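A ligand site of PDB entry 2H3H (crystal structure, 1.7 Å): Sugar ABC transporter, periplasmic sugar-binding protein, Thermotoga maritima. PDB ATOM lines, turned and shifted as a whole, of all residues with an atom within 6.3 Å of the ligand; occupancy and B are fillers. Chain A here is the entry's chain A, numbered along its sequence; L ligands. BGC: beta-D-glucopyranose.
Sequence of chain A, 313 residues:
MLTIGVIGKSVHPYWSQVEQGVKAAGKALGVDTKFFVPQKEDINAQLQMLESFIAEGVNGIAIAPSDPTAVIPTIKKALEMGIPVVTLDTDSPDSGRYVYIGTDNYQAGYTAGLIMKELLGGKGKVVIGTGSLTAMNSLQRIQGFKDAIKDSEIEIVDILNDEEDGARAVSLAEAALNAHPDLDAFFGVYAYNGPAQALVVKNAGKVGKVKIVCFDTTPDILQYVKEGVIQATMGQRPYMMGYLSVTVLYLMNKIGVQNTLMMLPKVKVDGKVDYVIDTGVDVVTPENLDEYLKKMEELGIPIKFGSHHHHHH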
ATOM      1  N   LYS A   9       9.561 -26.741  25.773  1.00  0.00           N
ATOM      2  CA  LYS A   9       8.773 -26.723  27.015  1.00  0.00           C
ATOM      3  C   LYS A   9       7.367 -26.082  26.920  1.00  0.00           C
ATOM      4  O   LYS A   9       6.481 -26.426  27.692  1.00  0.00           O
ATOM      5  CB  LYS A   9       9.577 -26.076  28.164  1.00  0.00           C
ATOM      6  CG  LYS A   9      10.780 -26.940  28.587  1.00  0.00           C
ATOM      7  CD  LYS A   9      11.873 -26.172  29.293  1.00  0.00           C
ATOM      8  CE  LYS A   9      11.528 -25.710  30.689  1.00  0.00           C
ATOM      9  NZ  LYS A   9      10.752 -24.439  30.698  1.00  0.00           N
ATOM     10  N   SER A  10       7.174 -25.177  25.982  1.00  0.00           N
ATOM     11  CA  SER A  10       5.857 -24.513  25.826  1.00  0.00           C
ATOM     12  C   SER A  10       5.760 -23.856  24.447  1.00  0.00           C
ATOM     13  O   SER A  10       6.734 -23.759  23.736  1.00  0.00           O
ATOM     14  CB  SER A  10       5.660 -23.458  26.900  1.00  0.00           C
ATOM     15  OG  SER A  10       6.524 -22.353  26.712  1.00  0.00           O
ATOM     16  N   HIS A  12       5.493 -20.764  23.632  1.00  0.00           N
ATOM     17  CA  HIS A  12       6.009 -19.387  23.532  1.00  0.00           C
ATOM     18  C   HIS A  12       6.870 -19.086  22.259  1.00  0.00           C
ATOM     19  O   HIS A  12       7.627 -19.977  21.792  1.00  0.00           O
ATOM     20  CB  HIS A  12       6.818 -19.041  24.769  1.00  0.00           C
ATOM     21  CG  HIS A  12       6.989 -17.570  24.975  1.00  0.00           C
ATOM     22  ND1 HIS A  12       8.025 -16.860  24.427  1.00  0.00           N
ATOM     23  CD2 HIS A  12       6.207 -16.669  25.609  1.00  0.00           C
ATOM     24  CE1 HIS A  12       7.884 -15.583  24.715  1.00  0.00           C
ATOM     25  NE2 HIS A  12       6.800 -15.437  25.439  1.00  0.00           N
ATOM     26  N   TYR A  14       9.609 -17.718  22.054  1.00  0.00           N
ATOM     27  CA  TYR A  14      10.926 -18.235  22.428  1.00  0.00           C
ATOM     28  C   TYR A  14      11.222 -19.595  21.805  1.00  0.00           C
ATOM     29  O   TYR A  14      12.332 -19.807  21.316  1.00  0.00           O
ATOM     30  CB  TYR A  14      11.048 -18.326  23.958  1.00  0.00           C
ATOM     31  CG  TYR A  14      12.361 -18.841  24.453  1.00  0.00           C
ATOM     32  CD1 TYR A  14      13.414 -17.958  24.735  1.00  0.00           C
ATOM     33  CD2 TYR A  14      12.569 -20.203  24.655  1.00  0.00           C
ATOM     34  CE1 TYR A  14      14.645 -18.432  25.145  1.00  0.00           C
ATOM     35  CE2 TYR A  14      13.791 -20.679  25.085  1.00  0.00           C
ATOM     36  CZ  TYR A  14      14.794 -19.795  25.366  1.00  0.00           C
ATOM     37  OH  TYR A  14      15.998 -20.297  25.794  1.00  0.00           O
ATOM     38  N   TRP A  15      10.270 -20.529  21.855  1.00  0.00           N
ATOM     39  CA  TRP A  15      10.518 -21.845  21.315  1.00  0.00           C
ATOM     40  C   TRP A  15      10.486 -21.873  19.781  1.00  0.00           C
ATOM     41  O   TRP A  15      11.127 -22.728  19.159  1.00  0.00           O
ATOM     42  CB  TRP A  15       9.594 -22.874  21.970  1.00  0.00           C
ATOM     43  CG  TRP A  15      10.083 -23.128  23.330  1.00  0.00           C
ATOM     44  CD1 TRP A  15       9.596 -22.655  24.493  1.00  0.00           C
ATOM     45  CD2 TRP A  15      11.283 -23.855  23.649  1.00  0.00           C
ATOM     46  NE1 TRP A  15      10.360 -23.088  25.560  1.00  0.00           N
ATOM     47  CE2 TRP A  15      11.412 -23.827  25.068  1.00  0.00           C
ATOM     48  CE3 TRP A  15      12.189 -24.577  22.892  1.00  0.00           C
ATOM     49  CZ2 TRP A  15      12.455 -24.461  25.735  1.00  0.00           C
ATOM     50  CZ3 TRP A  15      13.232 -25.207  23.550  1.00  0.00           C
ATOM     51  CH2 TRP A  15      13.345 -25.147  24.961  1.00  0.00           C
ATOM     52  N   ALA A  64      14.665 -30.271  26.433  1.00  0.00           N
ATOM     53  CA  ALA A  64      14.661 -29.272  27.482  1.00  0.00           C
ATOM     54  C   ALA A  64      13.673 -29.760  28.556  1.00  0.00           C
ATOM     55  O   ALA A  64      12.503 -29.384  28.556  1.00  0.00           O
ATOM     56  CB  ALA A  64      14.198 -27.939  26.924  1.00  0.00           C
ATOM     57  N   ASP A  89      18.574 -25.508  26.840  1.00  0.00           N
ATOM     58  CA  ASP A  89      17.777 -24.516  27.546  1.00  0.00           C
ATOM     59  C   ASP A  89      17.727 -24.752  29.069  1.00  0.00           C
ATOM     60  O   ASP A  89      17.775 -23.794  29.852  1.00  0.00           O
ATOM     61  CB  ASP A  89      16.392 -24.470  26.930  1.00  0.00           C
ATOM     62  CG  ASP A  89      15.421 -23.572  27.672  1.00  0.00           C
ATOM     63  OD1 ASP A  89      15.502 -22.344  27.493  1.00  0.00           O
ATOM     64  OD2 ASP A  89      14.579 -24.117  28.402  1.00  0.00           O
ATOM     65  N   THR A  90      17.506 -26.008  29.468  1.00  0.00           N
ATOM     66  CA  THR A  90      17.509 -26.442  30.874  1.00  0.00           C
ATOM     67  C   THR A  90      18.049 -27.877  30.955  1.00  0.00           C
ATOM     68  O   THR A  90      17.923 -28.653  29.995  1.00  0.00           O
ATOM     69  CB  THR A  90      16.085 -26.311  31.506  1.00  0.00           C
ATOM     70  OG1 THR A  90      16.144 -26.581  32.911  1.00  0.00           O
ATOM     71  CG2 THR A  90      15.107 -27.256  30.817  1.00  0.00           C
ATOM     72  N   ASN A 105      22.430 -20.418  33.719  1.00  0.00           N
ATOM     73  CA  ASN A 105      21.227 -19.877  34.335  1.00  0.00           C
ATOM     74  C   ASN A 105      21.466 -19.301  35.705  1.00  0.00           C
ATOM     75  O   ASN A 105      20.880 -18.271  36.046  1.00  0.00           O
ATOM     76  CB  ASN A 105      20.153 -20.962  34.389  1.00  0.00           C
ATOM     77  CG  ASN A 105      19.649 -21.313  33.025  1.00  0.00           C
ATOM     78  OD1 ASN A 105      19.020 -20.492  32.398  1.00  0.00           O
ATOM     79  ND2 ASN A 105      20.017 -22.495  32.518  1.00  0.00           N
ATOM     80  N   GLY A 131       7.573 -19.738  35.319  1.00  0.00           N
ATOM     81  CA  GLY A 131       6.729 -20.752  34.706  1.00  0.00           C
ATOM     82  C   GLY A 131       7.066 -22.185  35.114  1.00  0.00           C
ATOM     83  O   GLY A 131       6.532 -23.121  34.542  1.00  0.00           O
ATOM     84  N   ALA A 135      11.749 -27.099  36.729  1.00  0.00           N
ATOM     85  CA  ALA A 135      12.782 -27.003  35.715  1.00  0.00           C
ATOM     86  C   ALA A 135      14.032 -26.314  36.274  1.00  0.00           C
ATOM     87  O   ALA A 135      13.952 -25.289  36.915  1.00  0.00           O
ATOM     88  CB  ALA A 135      12.244 -26.263  34.456  1.00  0.00           C
ATOM     89  N   ASN A 137      16.497 -24.582  35.031  1.00  0.00           N
ATOM     90  CA  ASN A 137      16.816 -23.225  34.627  1.00  0.00           C
ATOM     91  C   ASN A 137      16.098 -22.182  35.491  1.00  0.00           C
ATOM     92  O   ASN A 137      16.702 -21.215  35.906  1.00  0.00           O
ATOM     93  CB  ASN A 137      16.631 -23.000  33.108  1.00  0.00           C
ATOM     94  CG  ASN A 137      15.195 -23.089  32.626  1.00  0.00           C
ATOM     95  OD1 ASN A 137      14.312 -23.730  33.224  1.00  0.00           O
ATOM     96  ND2 ASN A 137      14.969 -22.487  31.445  1.00  0.00           N
ATOM     97  N   ARG A 141      17.988 -19.665  38.047  1.00  0.00           N
ATOM     98  CA  ARG A 141      17.818 -18.235  37.898  1.00  0.00           C
ATOM     99  C   ARG A 141      17.351 -17.603  39.219  1.00  0.00           C
ATOM    100  O   ARG A 141      17.826 -16.548  39.621  1.00  0.00           O
ATOM    101  CB  ARG A 141      16.855 -17.874  36.754  1.00  0.00           C
ATOM    102  CG  ARG A 141      17.419 -18.181  35.373  1.00  0.00           C
ATOM    103  CD  ARG A 141      16.400 -18.034  34.275  1.00  0.00           C
ATOM    104  NE  ARG A 141      16.856 -18.767  33.095  1.00  0.00           N
ATOM    105  CZ  ARG A 141      16.146 -18.916  31.972  1.00  0.00           C
ATOM    106  NH1 ARG A 141      14.957 -18.345  31.837  1.00  0.00           N
ATOM    107  NH2 ARG A 141      16.652 -19.633  30.987  1.00  0.00           N
ATOM    108  N   GLU A 164       4.001 -21.728  32.613  1.00  0.00           N
ATOM    109  CA  GLU A 164       4.153 -21.342  31.206  1.00  0.00           C
ATOM    110  C   GLU A 164       2.809 -21.172  30.493  1.00  0.00           C
ATOM    111  O   GLU A 164       2.587 -21.704  29.405  1.00  0.00           O
ATOM    112  CB  GLU A 164       5.103 -22.320  30.461  1.00  0.00           C
ATOM    113  CG  GLU A 164       6.442 -22.493  31.161  1.00  0.00           C
ATOM    114  CD  GLU A 164       7.528 -23.004  30.256  1.00  0.00           C
ATOM    115  OE1 GLU A 164       7.791 -22.355  29.211  1.00  0.00           O
ATOM    116  OE2 GLU A 164       8.112 -24.080  30.562  1.00  0.00           O
ATOM    117  N   VAL A 189      11.192 -14.523  35.198  1.00  0.00           N
ATOM    118  CA  VAL A 189      12.192 -15.599  35.057  1.00  0.00           C
ATOM    119  C   VAL A 189      12.147 -16.248  33.666  1.00  0.00           C
ATOM    120  O   VAL A 189      13.198 -16.578  33.090  1.00  0.00           O
ATOM    121  CB  VAL A 189      11.998 -16.674  36.160  1.00  0.00           C
ATOM    122  CG1 VAL A 189      12.881 -17.901  35.903  1.00  0.00           C
ATOM    123  CG2 VAL A 189      12.256 -16.077  37.541  1.00  0.00           C
ATOM    124  N   TYR A 190      10.954 -16.461  33.154  1.00  0.00           N
ATOM    125  CA  TYR A 190      10.710 -17.044  31.835  1.00  0.00           C
ATOM    126  C   TYR A 190      10.182 -15.967  30.878  1.00  0.00           C
ATOM    127  O   TYR A 190       9.816 -14.856  31.300  1.00  0.00           O
ATOM    128  CB  TYR A 190       9.700 -18.183  31.946  1.00  0.00           C
ATOM    129  CG  TYR A 190      10.225 -19.529  32.392  1.00  0.00           C
ATOM    130  CD1 TYR A 190      11.569 -19.736  32.630  1.00  0.00           C
ATOM    131  CD2 TYR A 190       9.374 -20.643  32.457  1.00  0.00           C
ATOM    132  CE1 TYR A 190      12.042 -20.968  32.992  1.00  0.00           C
ATOM    133  CE2 TYR A 190       9.850 -21.896  32.798  1.00  0.00           C
ATOM    134  CZ  TYR A 190      11.193 -22.048  33.071  1.00  0.00           C
ATOM    135  OH  TYR A 190      11.708 -23.289  33.377  1.00  0.00           O
ATOM    136  N   ALA A 191      10.090 -16.306  29.598  1.00  0.00           N
ATOM    137  CA  ALA A 191       9.746 -15.345  28.556  1.00  0.00           C
ATOM    138  C   ALA A 191       8.340 -14.766  28.729  1.00  0.00           C
ATOM    139  O   ALA A 191       8.091 -13.642  28.311  1.00  0.00           O
ATOM    140  CB  ALA A 191       9.881 -15.968  27.198  1.00  0.00           C
ATOM    141  N   TYR A 192       7.422 -15.550  29.306  1.00  0.00           N
ATOM    142  CA  TYR A 192       6.059 -15.066  29.571  1.00  0.00           C
ATOM    143  C   TYR A 192       6.007 -13.945  30.628  1.00  0.00           C
ATOM    144  O   TYR A 192       5.073 -13.133  30.645  1.00  0.00           O
ATOM    145  CB  TYR A 192       5.140 -16.196  30.051  1.00  0.00           C
ATOM    146  CG  TYR A 192       4.645 -17.152  28.959  1.00  0.00           C
ATOM    147  CD1 TYR A 192       3.594 -16.775  28.113  1.00  0.00           C
ATOM    148  CD2 TYR A 192       5.215 -18.402  28.783  1.00  0.00           C
ATOM    149  CE1 TYR A 192       3.130 -17.640  27.128  1.00  0.00           C
ATOM    150  CE2 TYR A 192       4.766 -19.258  27.781  1.00  0.00           C
ATOM    151  CZ  TYR A 192       3.726 -18.876  26.960  1.00  0.00           C
ATOM    152  OH  TYR A 192       3.259 -19.707  25.968  1.00  0.00           O
ATOM    153  N   ASN A 193       6.970 -13.915  31.549  1.00  0.00           N
ATOM    154  CA  ASN A 193       6.819 -13.123  32.761  1.00  0.00           C
ATOM    155  C   ASN A 193       7.095 -11.639  32.608  1.00  0.00           C
ATOM    156  O   ASN A 193       6.277 -10.815  33.031  1.00  0.00           O
ATOM    157  CB  ASN A 193       7.653 -13.754  33.878  1.00  0.00           C
ATOM    158  CG  ASN A 193       7.203 -15.177  34.158  1.00  0.00           C
ATOM    159  OD1 ASN A 193       7.898 -16.146  33.817  1.00  0.00           O
ATOM    160  ND2 ASN A 193       6.008 -15.305  34.744  1.00  0.00           N
ATOM    161  N   PHE A 215      13.778 -11.883  31.790  1.00  0.00           N
ATOM    162  CA  PHE A 215      14.510 -12.688  30.846  1.00  0.00           C
ATOM    163  C   PHE A 215      13.958 -12.546  29.422  1.00  0.00           C
ATOM    164  O   PHE A 215      12.775 -12.268  29.214  1.00  0.00           O
ATOM    165  CB  PHE A 215      14.523 -14.147  31.301  1.00  0.00           C
ATOM    166  CG  PHE A 215      15.672 -14.472  32.186  1.00  0.00           C
ATOM    167  CD1 PHE A 215      16.746 -15.223  31.711  1.00  0.00           C
ATOM    168  CD2 PHE A 215      15.718 -13.961  33.484  1.00  0.00           C
ATOM    169  CE1 PHE A 215      17.833 -15.482  32.512  1.00  0.00           C
ATOM    170  CE2 PHE A 215      16.797 -14.218  34.297  1.00  0.00           C
ATOM    171  CZ  PHE A 215      17.880 -14.988  33.814  1.00  0.00           C
ATOM    172  N   ASP A 216      14.857 -12.756  28.463  1.00  0.00           N
ATOM    173  CA  ASP A 216      14.550 -12.939  27.043  1.00  0.00           C
ATOM    174  C   ASP A 216      14.324 -11.627  26.282  1.00  0.00           C
ATOM    175  O   ASP A 216      14.250 -10.541  26.873  1.00  0.00           O
ATOM    176  CB  ASP A 216      13.409 -13.957  26.848  1.00  0.00           C
ATOM    177  CG  ASP A 216      13.718 -15.275  27.502  1.00  0.00           C
ATOM    178  OD1 ASP A 216      14.840 -15.773  27.229  1.00  0.00           O
ATOM    179  OD2 ASP A 216      12.894 -15.794  28.321  1.00  0.00           O
ATOM    180  N   GLN A 236      18.815 -14.440  26.182  1.00  0.00           N
ATOM    181  CA  GLN A 236      19.481 -15.682  25.818  1.00  0.00           C
ATOM    182  C   GLN A 236      19.712 -15.784  24.289  1.00  0.00           C
ATOM    183  O   GLN A 236      19.414 -14.840  23.515  1.00  0.00           O
ATOM    184  CB  GLN A 236      18.642 -16.871  26.331  1.00  0.00           C
ATOM    185  CG  GLN A 236      18.236 -16.809  27.789  1.00  0.00           C
ATOM    186  CD  GLN A 236      17.568 -18.111  28.208  1.00  0.00           C
ATOM    187  OE1 GLN A 236      18.250 -19.120  28.406  1.00  0.00           O
ATOM    188  NE2 GLN A 236      16.238 -18.119  28.238  1.00  0.00           N
ATOM    189  N   MET A 241      20.885 -22.312  20.611  1.00  0.00           N
ATOM    190  CA  MET A 241      20.550 -23.573  21.308  1.00  0.00           C
ATOM    191  C   MET A 241      20.031 -24.639  20.341  1.00  0.00           C
ATOM    192  O   MET A 241      20.528 -25.766  20.357  1.00  0.00           O
ATOM    193  CB  MET A 241      19.547 -23.337  22.425  1.00  0.00           C
ATOM    194  CG  MET A 241      20.107 -22.577  23.632  1.00  0.00           C
ATOM    195  SD  MET A 241      18.789 -22.122  24.772  1.00  0.00           S
ATOM    196  CE  MET A 241      19.381 -20.585  25.479  1.00  0.00           C
HETATM  197  C2  BGC L   1      13.229 -20.386  29.292  1.00  0.00           C
HETATM  198  C3  BGC L   1      12.412 -21.580  28.798  1.00  0.00           C
HETATM  199  C4  BGC L   1      10.883 -21.314  28.849  1.00  0.00           C
HETATM  200  C5  BGC L   1      10.674 -20.025  28.079  1.00  0.00           C
HETATM  201  C6  BGC L   1       9.194 -19.641  27.889  1.00  0.00           C
HETATM  202  C1  BGC L   1      12.710 -19.058  28.728  1.00  0.00           C
HETATM  203  O1  BGC L   1      13.216 -17.970  29.442  1.00  0.00           O
HETATM  204  O2  BGC L   1      14.651 -20.515  29.032  1.00  0.00           O
HETATM  205  O3  BGC L   1      12.811 -22.754  29.488  1.00  0.00           O
HETATM  206  O4  BGC L   1      10.160 -22.448  28.355  1.00  0.00           O
HETATM  207  O5  BGC L   1      11.311 -18.993  28.819  1.00  0.00           O
HETATM  208  O6  BGC L   1       8.520 -19.625  29.136  1.00  0.00           O
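OD2 of Asp 216 is in hydrogen-bond range of O1 of the ligand (2.5 Å). OD2 of Asp 89 sits at hydrogen-bond distance from O3 of the ligand. OE1 of Glu 164 sits at hydrogen-bond distance from O4 of the ligand, at 2.5 Å. The indole nitrogen of Trp 15 is in hydrogen-bond range of an oxygen (O4) of the ligand (2.9 Å). NZ of Lys 9 is in hydrogen-bond range of O3 of the ligand (2.9 Å). An oxygen (O3) of the ligand lies within hydrogen-bond range of the side-chain amide nitrogen (ND2) of Asn 137 (2.9 Å). An oxygen (O2) of the ligand sits at hydrogen-bond distance from the guanidinium group (NH2) of Arg 141 (2.9 Å). An oxygen (O2) of the ligand lies within hydrogen-bond range of the side-chain amide nitrogen (NE2) of Gln 236, 3.0 Å away. The backbone NH of Ala 191 sits at hydrogen-bond distance from an oxygen (O5) of the ligand (3.1 Å).
The side-chain amide nitrogen (NE2) of Gln 236 is in hydrogen-bond range of the side-chain carboxylate (OD1) of Asp 216 (2.9 Å). OD1 of Asp 89 lies within hydrogen-bond range of OH of Tyr 14 (2.7 Å). OE2 of Glu 164 is in salt-bridge range of NZ of Lys 9 (2.7 Å). The side-chain carboxylate (OE1) of Glu 164 is in hydrogen-bond range of the side-chain hydroxyl (OG) of Ser 10, at 2.8 Å. The side-chain amide nitrogen of Asn 137 lies close to the guanidinium group of Arg 141 (3.3 Å). The side-chain amide oxygen (OD1) of Asn 137 lies within hydrogen-bond range of the side-chain hydroxyl (OH) of Tyr 190 (2.6 Å). The side-chain amide oxygen of Asn 105 is in hydrogen-bond range of the guanidinium group of Arg 141 (2.9 Å). N of His 12 is in hydrogen-bond range of OH of Tyr 192 (3.4 Å).
OG of Ser 10 touches C6 of the ligand (3.98 Å). His 12 touches the ligand (CB to C6, 3.97 Å). Tyr 14 touches the ligand. Val 189 touches the ligand (O to O1, 3.9 Å). Tyr 190 touches the ligand. Tyr 192 touches the ligand. Hydrophobic or aromatic side chains that line the ligand: His 12, Tyr 14, Trp 15, Tyr 190, Ala 191 and Tyr 192. Along chain A the residues within 4 Å of the ligand span positions 9 to 236.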
